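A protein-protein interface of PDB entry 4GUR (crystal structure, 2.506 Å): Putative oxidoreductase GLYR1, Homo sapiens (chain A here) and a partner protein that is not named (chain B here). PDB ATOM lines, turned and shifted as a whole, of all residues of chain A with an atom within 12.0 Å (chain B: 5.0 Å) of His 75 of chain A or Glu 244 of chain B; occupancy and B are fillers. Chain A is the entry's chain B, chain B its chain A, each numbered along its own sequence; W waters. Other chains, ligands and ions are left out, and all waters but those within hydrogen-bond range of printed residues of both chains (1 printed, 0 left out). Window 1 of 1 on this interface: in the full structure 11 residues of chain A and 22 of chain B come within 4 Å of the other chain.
OD1 of Asp 246 of chain B sits at hydrogen-bond distance from N of Gln 80 of chain A (3.1 Å). The backbone NH of Asp 246 of chain B sits at hydrogen-bond distance from the backbone carbonyl oxygen of Leu 78 of chain A, at 3.0 Å. OD1 of Asp 246 of chain B is in hydrogen-bond range of N of Thr 81 of chain A, at 2.9 Å. The backbone NH of His 75 of chain A is in hydrogen-bond range of the side-chain carboxylate of Glu 244 of chain B (2.9 Å).
The backbone NH (N) of Arg 239 of chain B lies within hydrogen-bond range of the side-chain carboxylate (OE1) of Glu 244 of chain B. The backbone carbonyl oxygen of His 75 of chain A lies within hydrogen-bond range of the side-chain hydroxyl of Ser 79 of chain A. The side-chain amide nitrogen (NE2) of Gln 80 of chain A lies within hydrogen-bond range of the backbone carbonyl oxygen (O) of Phe 76 of chain A (3.0 Å). The side-chain carboxylate (OE2) of Glu 247 of chain B is in salt-bridge range of the guanidinium group (NE) of Arg 265 of chain B. The side-chain carboxylate (OE1) of Glu 247 of chain B sits at hydrogen-bond distance from the backbone NH (N) of Glu 244 of chain B (2.6 Å). A ring nitrogen (ND1) of His 75 of chain A lies within hydrogen-bond range of the backbone NH (N) of Leu 77 of chain A (3.0 Å).
Among the printed residues, merely in contact across the chains: His 75 of chain A with Leu 236 of chain B (3.2 Å), His 75 of chain A with Leu 315 of chain B (3.2 Å), Ser 79 of chain A with Asp 246 of chain B (3.5 Å), His 75 of chain A with Cys 237 of chain B (3.5 Å), Leu 77 of chain A with Asp 246 of chain B (3.5 Å), His 74 of chain A with Glu 244 of chain B (3.6 Å), His 75 of chain A with Val 238 of chain B (3.6 Å), Leu 77 of chain A with Leu 315 of chain B (3.7 Å), Leu 78 of chain A with Leu 245 of chain B (3.8 Å), Phe 76 of chain A with Leu 236 of chain B (3.8 Å), Leu 78 of chain A with Leu 315 of chain B (3.8 Å), Leu 78 of chain A with Glu 247 of chain B (3.9 Å) and Leu 78 of chain A with Glu 244 of chain B (3.96 Å).
His 75 of chain A touches just these residues of chain B: Leu 236 (3.2 Å), Cys 237 (3.5 Å), Val 238 (3.6 Å), Glu 244 (2.9 Å) and Leu 315 (3.2 Å). Glu 244 of chain B touches just these residues of chain A: His 74, His 75 and Leu 78. Leu 236 of chain B touches two residues of chain A. Cys 237 of chain B touches just one residue of chain A: His 75. Of chain A, only His 75 comes within 4 Å of Val 238 of chain B. No residue of chain A comes within 4 Å of Val 242 of chain B. Asp 246 of chain B touches just these residues of chain A: Leu 77, Leu 78, Ser 79, Gln 80 and Thr 81. Of chain A, only His 75, Leu 77 and Leu 78 come within 4 Å of Leu 315 of chain B. Printed residues of chain B within 4 Å of Ser 79 of chain A: Asp 246 (3.5 Å). Of the printed residues of chain B, Leu 78 of chain A touches Glu 244, Leu 245, Asp 246, Glu 247 and Leu 315. Of the printed residues of chain B, Gln 80 of chain A touches Asp 246 (3.1 Å). Printed residues of chain B within 4 Å of Leu 77 of chain A: Asp 246 (3.5 Å) and Leu 315 (3.7 Å). Of the printed residues of chain B, Thr 81 of chain A touches Asp 246 (2.9 Å). Arg 239 of chain B touches none of the printed residues of chain A. Phe 73 of chain A touches none of the printed residues of chain B. The nearest printed residue of chain B that does not touch His 75 of chain A is Arg 239 of chain B (6.6 Å). The nearest printed residue of chain B that does not touch Thr 81 of chain A is Leu 245 of chain B (4.5 Å).
Of the 13 printed residues of chain B, 8 touch a printed residue of chain A. Hydrophobic or aromatic side chains of chain B within 4 Å of the printed part of chain A: Leu 236, Val 238 and Leu 315. Of the 12 printed residues of chain A, 8 touch a printed residue of chain B. Hydrophobic or aromatic side chains of chain A that line the printed part of chain B: His 74, His 75, Phe 76, Leu 77 and Leu 78. Among the printed residues, 17 pairs touch across the chains.
Water W1 lies within hydrogen-bond range of N of Leu 236 of chain B (2.8 Å), O of His 74 of chain A (3.2 Å) and N of Phe 76 of chain A (3.2 Å).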
ATOM      1  N   ASP A  70      28.196 -16.831 -22.824  1.00  0.00           N
ATOM      2  CA  ASP A  70      27.715 -18.056 -23.528  1.00  0.00           C
ATOM      3  C   ASP A  70      26.680 -17.696 -24.599  1.00  0.00           C
ATOM      4  O   ASP A  70      25.554 -17.298 -24.268  1.00  0.00           O
ATOM      5  CB  ASP A  70      27.132 -19.065 -22.528  1.00  0.00           C
ATOM      6  CG  ASP A  70      26.950 -20.458 -23.127  1.00  0.00           C
ATOM      7  OD1 ASP A  70      27.109 -20.628 -24.361  1.00  0.00           O
ATOM      8  OD2 ASP A  70      26.645 -21.392 -22.354  1.00  0.00           O
ATOM      9  N   PRO A  71      27.056 -17.851 -25.886  1.00  0.00           N
ATOM     10  CA  PRO A  71      26.195 -17.459 -27.013  1.00  0.00           C
ATOM     11  C   PRO A  71      24.956 -18.351 -27.208  1.00  0.00           C
ATOM     12  O   PRO A  71      24.021 -17.951 -27.914  1.00  0.00           O
ATOM     13  CB  PRO A  71      27.127 -17.559 -28.237  1.00  0.00           C
ATOM     14  CG  PRO A  71      28.493 -17.861 -27.710  1.00  0.00           C
ATOM     15  CD  PRO A  71      28.316 -18.461 -26.349  1.00  0.00           C
ATOM     16  N   HIS A  72      24.942 -19.531 -26.586  1.00  0.00           N
ATOM     17  CA  HIS A  72      23.815 -20.460 -26.721  1.00  0.00           C
ATOM     18  C   HIS A  72      22.503 -19.866 -26.271  1.00  0.00           C
ATOM     19  O   HIS A  72      21.476 -20.077 -26.920  1.00  0.00           O
ATOM     20  CB  HIS A  72      24.087 -21.775 -25.981  1.00  0.00           C
ATOM     21  CG  HIS A  72      22.910 -22.740 -25.988  1.00  0.00           C
ATOM     22  ND1 HIS A  72      22.579 -23.480 -27.068  1.00  0.00           N
ATOM     23  CD2 HIS A  72      21.980 -23.062 -24.994  1.00  0.00           C
ATOM     24  CE1 HIS A  72      21.502 -24.238 -26.782  1.00  0.00           C
ATOM     25  NE2 HIS A  72      21.138 -23.983 -25.514  1.00  0.00           N
ATOM     26  N   PHE A  73      22.540 -19.109 -25.170  1.00  0.00           N
ATOM     27  CA  PHE A  73      21.330 -18.604 -24.502  1.00  0.00           C
ATOM     28  C   PHE A  73      20.764 -17.280 -25.048  1.00  0.00           C
ATOM     29  O   PHE A  73      19.548 -17.069 -25.044  1.00  0.00           O
ATOM     30  CB  PHE A  73      21.569 -18.500 -22.990  1.00  0.00           C
ATOM     31  CG  PHE A  73      21.764 -19.830 -22.315  1.00  0.00           C
ATOM     32  CD1 PHE A  73      20.669 -20.568 -21.871  1.00  0.00           C
ATOM     33  CD2 PHE A  73      23.043 -20.346 -22.120  1.00  0.00           C
ATOM     34  CE1 PHE A  73      20.843 -21.793 -21.243  1.00  0.00           C
ATOM     35  CE2 PHE A  73      23.223 -21.573 -21.502  1.00  0.00           C
ATOM     36  CZ  PHE A  73      22.122 -22.297 -21.062  1.00  0.00           C
ATOM     37  N   HIS A  74      21.654 -16.408 -25.515  1.00  0.00           N
ATOM     38  CA  HIS A  74      21.300 -15.088 -26.033  1.00  0.00           C
ATOM     39  C   HIS A  74      20.084 -14.997 -26.929  1.00  0.00           C
ATOM     40  O   HIS A  74      19.905 -15.774 -27.880  1.00  0.00           O
ATOM     41  CB  HIS A  74      22.490 -14.472 -26.761  1.00  0.00           C
ATOM     42  CG  HIS A  74      23.684 -14.205 -25.879  1.00  0.00           C
ATOM     43  ND1 HIS A  74      23.572 -13.918 -24.563  1.00  0.00           N
ATOM     44  CD2 HIS A  74      25.048 -14.158 -26.180  1.00  0.00           C
ATOM     45  CE1 HIS A  74      24.799 -13.716 -24.044  1.00  0.00           C
ATOM     46  NE2 HIS A  74      25.702 -13.863 -25.037  1.00  0.00           N
ATOM     47  N   HIS A  75      19.245 -14.013 -26.622  1.00  0.00           N
ATOM     48  CA  HIS A  75      18.110 -13.653 -27.456  1.00  0.00           C
ATOM     49  C   HIS A  75      18.566 -13.212 -28.828  1.00  0.00           C
ATOM     50  O   HIS A  75      19.377 -12.292 -28.970  1.00  0.00           O
ATOM     51  CB  HIS A  75      17.322 -12.545 -26.777  1.00  0.00           C
ATOM     52  CG  HIS A  75      15.998 -12.252 -27.426  1.00  0.00           C
ATOM     53  ND1 HIS A  75      15.898 -11.679 -28.638  1.00  0.00           N
ATOM     54  CD2 HIS A  75      14.695 -12.454 -26.974  1.00  0.00           C
ATOM     55  CE1 HIS A  75      14.597 -11.541 -28.959  1.00  0.00           C
ATOM     56  NE2 HIS A  75      13.863 -12.012 -27.937  1.00  0.00           N
ATOM     57  N   PHE A  76      18.038 -13.882 -29.846  1.00  0.00           N
ATOM     58  CA  PHE A  76      18.411 -13.658 -31.245  1.00  0.00           C
ATOM     59  C   PHE A  76      18.398 -12.182 -31.695  1.00  0.00           C
ATOM     60  O   PHE A  76      19.278 -11.759 -32.455  1.00  0.00           O
ATOM     61  CB  PHE A  76      17.537 -14.526 -32.171  1.00  0.00           C
ATOM     62  CG  PHE A  76      17.809 -14.321 -33.639  1.00  0.00           C
ATOM     63  CD1 PHE A  76      18.947 -14.872 -34.236  1.00  0.00           C
ATOM     64  CD2 PHE A  76      16.926 -13.572 -34.429  1.00  0.00           C
ATOM     65  CE1 PHE A  76      19.197 -14.676 -35.585  1.00  0.00           C
ATOM     66  CE2 PHE A  76      17.172 -13.374 -35.782  1.00  0.00           C
ATOM     67  CZ  PHE A  76      18.307 -13.929 -36.360  1.00  0.00           C
ATOM     68  N   LEU A  77      17.422 -11.404 -31.222  1.00  0.00           N
ATOM     69  CA  LEU A  77      17.277 -10.017 -31.672  1.00  0.00           C
ATOM     70  C   LEU A  77      18.137  -9.001 -30.912  1.00  0.00           C
ATOM     71  O   LEU A  77      18.312  -7.858 -31.369  1.00  0.00           O
ATOM     72  CB  LEU A  77      15.805  -9.592 -31.678  1.00  0.00           C
ATOM     73  CG  LEU A  77      14.883 -10.307 -32.679  1.00  0.00           C
ATOM     74  CD1 LEU A  77      13.470  -9.767 -32.557  1.00  0.00           C
ATOM     75  CD2 LEU A  77      15.374 -10.219 -34.132  1.00  0.00           C
ATOM     76  N   LEU A  78      18.688  -9.427 -29.774  1.00  0.00           N
ATOM     77  CA  LEU A  78      19.511  -8.568 -28.926  1.00  0.00           C
ATOM     78  C   LEU A  78      20.974  -9.030 -28.877  1.00  0.00           C
ATOM     79  O   LEU A  78      21.720  -8.689 -27.944  1.00  0.00           O
ATOM     80  CB  LEU A  78      18.923  -8.504 -27.515  1.00  0.00           C
ATOM     81  CG  LEU A  78      17.541  -7.872 -27.323  1.00  0.00           C
ATOM     82  CD1 LEU A  78      17.124  -7.979 -25.863  1.00  0.00           C
ATOM     83  CD2 LEU A  78      17.523  -6.423 -27.782  1.00  0.00           C
ATOM     84  N   SER A  79      21.376  -9.799 -29.890  1.00  0.00           N
ATOM     85  CA  SER A  79      22.750 -10.293 -30.002  1.00  0.00           C
ATOM     86  C   SER A  79      23.400  -9.915 -31.325  1.00  0.00           C
ATOM     87  O   SER A  79      24.405 -10.502 -31.713  1.00  0.00           O
ATOM     88  CB  SER A  79      22.799 -11.809 -29.805  1.00  0.00           C
ATOM     89  OG  SER A  79      22.690 -12.126 -28.432  1.00  0.00           O
ATOM     90  N   GLN A  80      22.835  -8.919 -32.001  1.00  0.00           N
ATOM     91  CA  GLN A  80      23.349  -8.463 -33.294  1.00  0.00           C
ATOM     92  C   GLN A  80      24.451  -7.404 -33.132  1.00  0.00           C
ATOM     93  O   GLN A  80      24.641  -6.563 -34.011  1.00  0.00           O
ATOM     94  CB  GLN A  80      22.197  -7.940 -34.167  1.00  0.00           C
ATOM     95  CG  GLN A  80      21.028  -8.914 -34.335  1.00  0.00           C
ATOM     96  CD  GLN A  80      21.318 -10.070 -35.294  1.00  0.00           C
ATOM     97  OE1 GLN A  80      22.146  -9.957 -36.203  1.00  0.00           O
ATOM     98  NE2 GLN A  80      20.616 -11.187 -35.102  1.00  0.00           N
ATOM     99  N   THR A  81      25.183  -7.490 -32.012  1.00  0.00           N
ATOM    100  CA  THR A  81      26.205  -6.511 -31.556  1.00  0.00           C
ATOM    101  C   THR A  81      26.303  -5.216 -32.376  1.00  0.00           C
ATOM    102  O   THR A  81      25.787  -4.171 -31.972  1.00  0.00           O
ATOM    103  CB  THR A  81      27.621  -7.135 -31.397  1.00  0.00           C
ATOM    104  OG1 THR A  81      28.446  -6.784 -32.517  1.00  0.00           O
ATOM    105  CG2 THR A  81      27.561  -8.663 -31.230  1.00  0.00           C
ATOM    106  N   LEU B 236      14.450 -16.829 -28.109  1.00  0.00           N
ATOM    107  CA  LEU B 236      13.751 -15.547 -27.847  1.00  0.00           C
ATOM    108  C   LEU B 236      13.404 -15.301 -26.374  1.00  0.00           C
ATOM    109  O   LEU B 236      12.389 -14.687 -26.031  1.00  0.00           O
ATOM    110  CB  LEU B 236      12.530 -15.370 -28.759  1.00  0.00           C
ATOM    111  CG  LEU B 236      12.737 -15.487 -30.274  1.00  0.00           C
ATOM    112  CD1 LEU B 236      11.628 -14.760 -31.029  1.00  0.00           C
ATOM    113  CD2 LEU B 236      14.104 -14.977 -30.718  1.00  0.00           C
ATOM    114  N   CYS B 237      14.272 -15.794 -25.513  1.00  0.00           N
ATOM    115  CA  CYS B 237      14.137 -15.658 -24.088  1.00  0.00           C
ATOM    116  C   CYS B 237      15.176 -14.641 -23.675  1.00  0.00           C
ATOM    117  O   CYS B 237      16.298 -14.672 -24.201  1.00  0.00           O
ATOM    118  CB  CYS B 237      14.496 -16.982 -23.461  1.00  0.00           C
ATOM    119  SG  CYS B 237      13.225 -17.625 -22.395  1.00  0.00           S
ATOM    120  N   VAL B 238      14.817 -13.728 -22.773  1.00  0.00           N
ATOM    121  CA  VAL B 238      15.823 -12.850 -22.166  1.00  0.00           C
ATOM    122  C   VAL B 238      16.057 -13.225 -20.719  1.00  0.00           C
ATOM    123  O   VAL B 238      15.199 -13.814 -20.073  1.00  0.00           O
ATOM    124  CB  VAL B 238      15.496 -11.338 -22.277  1.00  0.00           C
ATOM    125  CG1 VAL B 238      15.303 -10.921 -23.732  1.00  0.00           C
ATOM    126  CG2 VAL B 238      14.304 -10.941 -21.406  1.00  0.00           C
ATOM    127  N   ARG B 239      17.239 -12.894 -20.220  1.00  0.00           N
ATOM    128  CA  ARG B 239      17.499 -12.975 -18.786  1.00  0.00           C
ATOM    129  C   ARG B 239      16.901 -11.718 -18.139  1.00  0.00           C
ATOM    130  O   ARG B 239      17.273 -10.588 -18.494  1.00  0.00           O
ATOM    131  CB  ARG B 239      19.005 -13.039 -18.494  1.00  0.00           C
ATOM    132  CG  ARG B 239      19.846 -13.875 -19.451  1.00  0.00           C
ATOM    133  CD  ARG B 239      19.865 -15.336 -19.050  1.00  0.00           C
ATOM    134  NE  ARG B 239      20.352 -15.536 -17.685  1.00  0.00           N
ATOM    135  CZ  ARG B 239      19.575 -15.765 -16.625  1.00  0.00           C
ATOM    136  NH1 ARG B 239      18.251 -15.824 -16.756  1.00  0.00           N
ATOM    137  NH2 ARG B 239      20.123 -15.933 -15.425  1.00  0.00           N
ATOM    138  N   VAL B 242      19.929  -9.863 -16.098  1.00  0.00           N
ATOM    139  CA  VAL B 242      21.188  -9.557 -16.785  1.00  0.00           C
ATOM    140  C   VAL B 242      20.867  -8.865 -18.104  1.00  0.00           C
ATOM    141  O   VAL B 242      19.965  -9.301 -18.820  1.00  0.00           O
ATOM    142  CB  VAL B 242      21.976 -10.856 -17.109  1.00  0.00           C
ATOM    143  CG1 VAL B 242      23.324 -10.528 -17.735  1.00  0.00           C
ATOM    144  CG2 VAL B 242      22.158 -11.716 -15.867  1.00  0.00           C
ATOM    145  N   MET B 243      21.596  -7.805 -18.441  1.00  0.00           N
ATOM    146  CA  MET B 243      21.460  -7.172 -19.764  1.00  0.00           C
ATOM    147  C   MET B 243      22.130  -8.027 -20.849  1.00  0.00           C
ATOM    148  O   MET B 243      23.139  -8.689 -20.591  1.00  0.00           O
ATOM    149  CB  MET B 243      22.059  -5.761 -19.777  1.00  0.00           C
ATOM    150  CG  MET B 243      21.253  -4.732 -19.001  1.00  0.00           C
ATOM    151  SD  MET B 243      22.078  -3.141 -18.739  1.00  0.00           S
ATOM    152  CE  MET B 243      21.630  -2.262 -20.228  1.00  0.00           C
ATOM    153  N   GLU B 244      21.557  -8.006 -22.052  1.00  0.00           N
ATOM    154  CA  GLU B 244      22.076  -8.731 -23.207  1.00  0.00           C
ATOM    155  C   GLU B 244      22.964  -7.765 -23.987  1.00  0.00           C
ATOM    156  O   GLU B 244      22.860  -6.550 -23.813  1.00  0.00           O
ATOM    157  CB  GLU B 244      20.931  -9.234 -24.107  1.00  0.00           C
ATOM    158  CG  GLU B 244      19.783  -9.966 -23.402  1.00  0.00           C
ATOM    159  CD  GLU B 244      19.726 -11.476 -23.656  1.00  0.00           C
ATOM    160  OE1 GLU B 244      19.241 -12.207 -22.762  1.00  0.00           O
ATOM    161  OE2 GLU B 244      20.139 -11.949 -24.737  1.00  0.00           O
ATOM    162  N   LEU B 245      23.816  -8.314 -24.854  1.00  0.00           N
ATOM    163  CA  LEU B 245      24.840  -7.553 -25.568  1.00  0.00           C
ATOM    164  C   LEU B 245      24.375  -6.287 -26.283  1.00  0.00           C
ATOM    165  O   LEU B 245      25.063  -5.280 -26.226  1.00  0.00           O
ATOM    166  CB  LEU B 245      25.592  -8.455 -26.557  1.00  0.00           C
ATOM    167  CG  LEU B 245      26.391  -9.650 -25.999  1.00  0.00           C
ATOM    168  CD1 LEU B 245      27.037 -10.448 -27.127  1.00  0.00           C
ATOM    169  CD2 LEU B 245      27.433  -9.229 -24.964  1.00  0.00           C
ATOM    170  N   ASP B 246      23.232  -6.310 -26.961  1.00  0.00           N
ATOM    171  CA  ASP B 246      22.820  -5.106 -27.692  1.00  0.00           C
ATOM    172  C   ASP B 246      22.353  -4.029 -26.734  1.00  0.00           C
ATOM    173  O   ASP B 246      22.426  -2.845 -27.050  1.00  0.00           O
ATOM    174  CB  ASP B 246      21.722  -5.391 -28.720  1.00  0.00           C
ATOM    175  CG  ASP B 246      22.213  -6.207 -29.916  1.00  0.00           C
ATOM    176  OD1 ASP B 246      23.325  -6.791 -29.855  1.00  0.00           O
ATOM    177  OD2 ASP B 246      21.455  -6.280 -30.917  1.00  0.00           O
ATOM    178  N   GLU B 247      21.865  -4.451 -25.568  1.00  0.00           N
ATOM    179  CA  GLU B 247      21.424  -3.535 -24.518  1.00  0.00           C
ATOM    180  C   GLU B 247      22.622  -2.859 -23.861  1.00  0.00           C
ATOM    181  O   GLU B 247      22.609  -1.642 -23.649  1.00  0.00           O
ATOM    182  CB  GLU B 247      20.595  -4.269 -23.455  1.00  0.00           C
ATOM    183  CG  GLU B 247      19.371  -5.007 -23.970  1.00  0.00           C
ATOM    184  CD  GLU B 247      18.699  -5.841 -22.889  1.00  0.00           C
ATOM    185  OE1 GLU B 247      19.380  -6.670 -22.248  1.00  0.00           O
ATOM    186  OE2 GLU B 247      17.481  -5.682 -22.673  1.00  0.00           O
ATOM    187  N   LEU B 248      23.646  -3.650 -23.522  1.00  0.00           N
ATOM    188  CA  LEU B 248      24.906  -3.104 -23.006  1.00  0.00           C
ATOM    189  C   LEU B 248      25.530  -2.133 -24.017  1.00  0.00           C
ATOM    190  O   LEU B 248      26.065  -1.102 -23.633  1.00  0.00           O
ATOM    191  CB  LEU B 248      25.911  -4.213 -22.682  1.00  0.00           C
ATOM    192  CG  LEU B 248      26.112  -4.902 -21.319  1.00  0.00           C
ATOM    193  CD1 LEU B 248      25.708  -4.038 -20.128  1.00  0.00           C
ATOM    194  CD2 LEU B 248      25.414  -6.252 -21.277  1.00  0.00           C
ATOM    195  N   ARG B 265      12.792  -2.495 -18.698  1.00  0.00           N
ATOM    196  CA  ARG B 265      12.735  -3.401 -19.842  1.00  0.00           C
ATOM    197  C   ARG B 265      11.757  -4.542 -19.537  1.00  0.00           C
ATOM    198  O   ARG B 265      10.877  -4.818 -20.353  1.00  0.00           O
ATOM    199  CB  ARG B 265      14.139  -3.901 -20.237  1.00  0.00           C
ATOM    200  CG  ARG B 265      14.191  -4.940 -21.363  1.00  0.00           C
ATOM    201  CD  ARG B 265      14.333  -6.359 -20.796  1.00  0.00           C
ATOM    202  NE  ARG B 265      15.731  -6.812 -20.799  1.00  0.00           N
ATOM    203  CZ  ARG B 265      16.230  -7.800 -20.057  1.00  0.00           C
ATOM    204  NH1 ARG B 265      15.472  -8.462 -19.192  1.00  0.00           N
ATOM    205  NH2 ARG B 265      17.514  -8.110 -20.179  1.00  0.00           N
ATOM    206  N   LEU B 315      11.373  -6.441 -30.564  1.00  0.00           N
ATOM    207  CA  LEU B 315      10.970  -7.175 -29.361  1.00  0.00           C
ATOM    208  C   LEU B 315       9.530  -6.904 -28.964  1.00  0.00           C
ATOM    209  O   LEU B 315       8.857  -7.766 -28.385  1.00  0.00           O
ATOM    210  CB  LEU B 315      11.874  -6.815 -28.184  1.00  0.00           C
ATOM    211  CG  LEU B 315      13.211  -7.520 -27.930  1.00  0.00           C
ATOM    212  CD1 LEU B 315      12.980  -8.963 -27.535  1.00  0.00           C
ATOM    213  CD2 LEU B 315      14.144  -7.436 -29.112  1.00  0.00           C
HETATM  214  O   HOH W   1      17.131 -16.871 -29.054  1.00  0.00           O
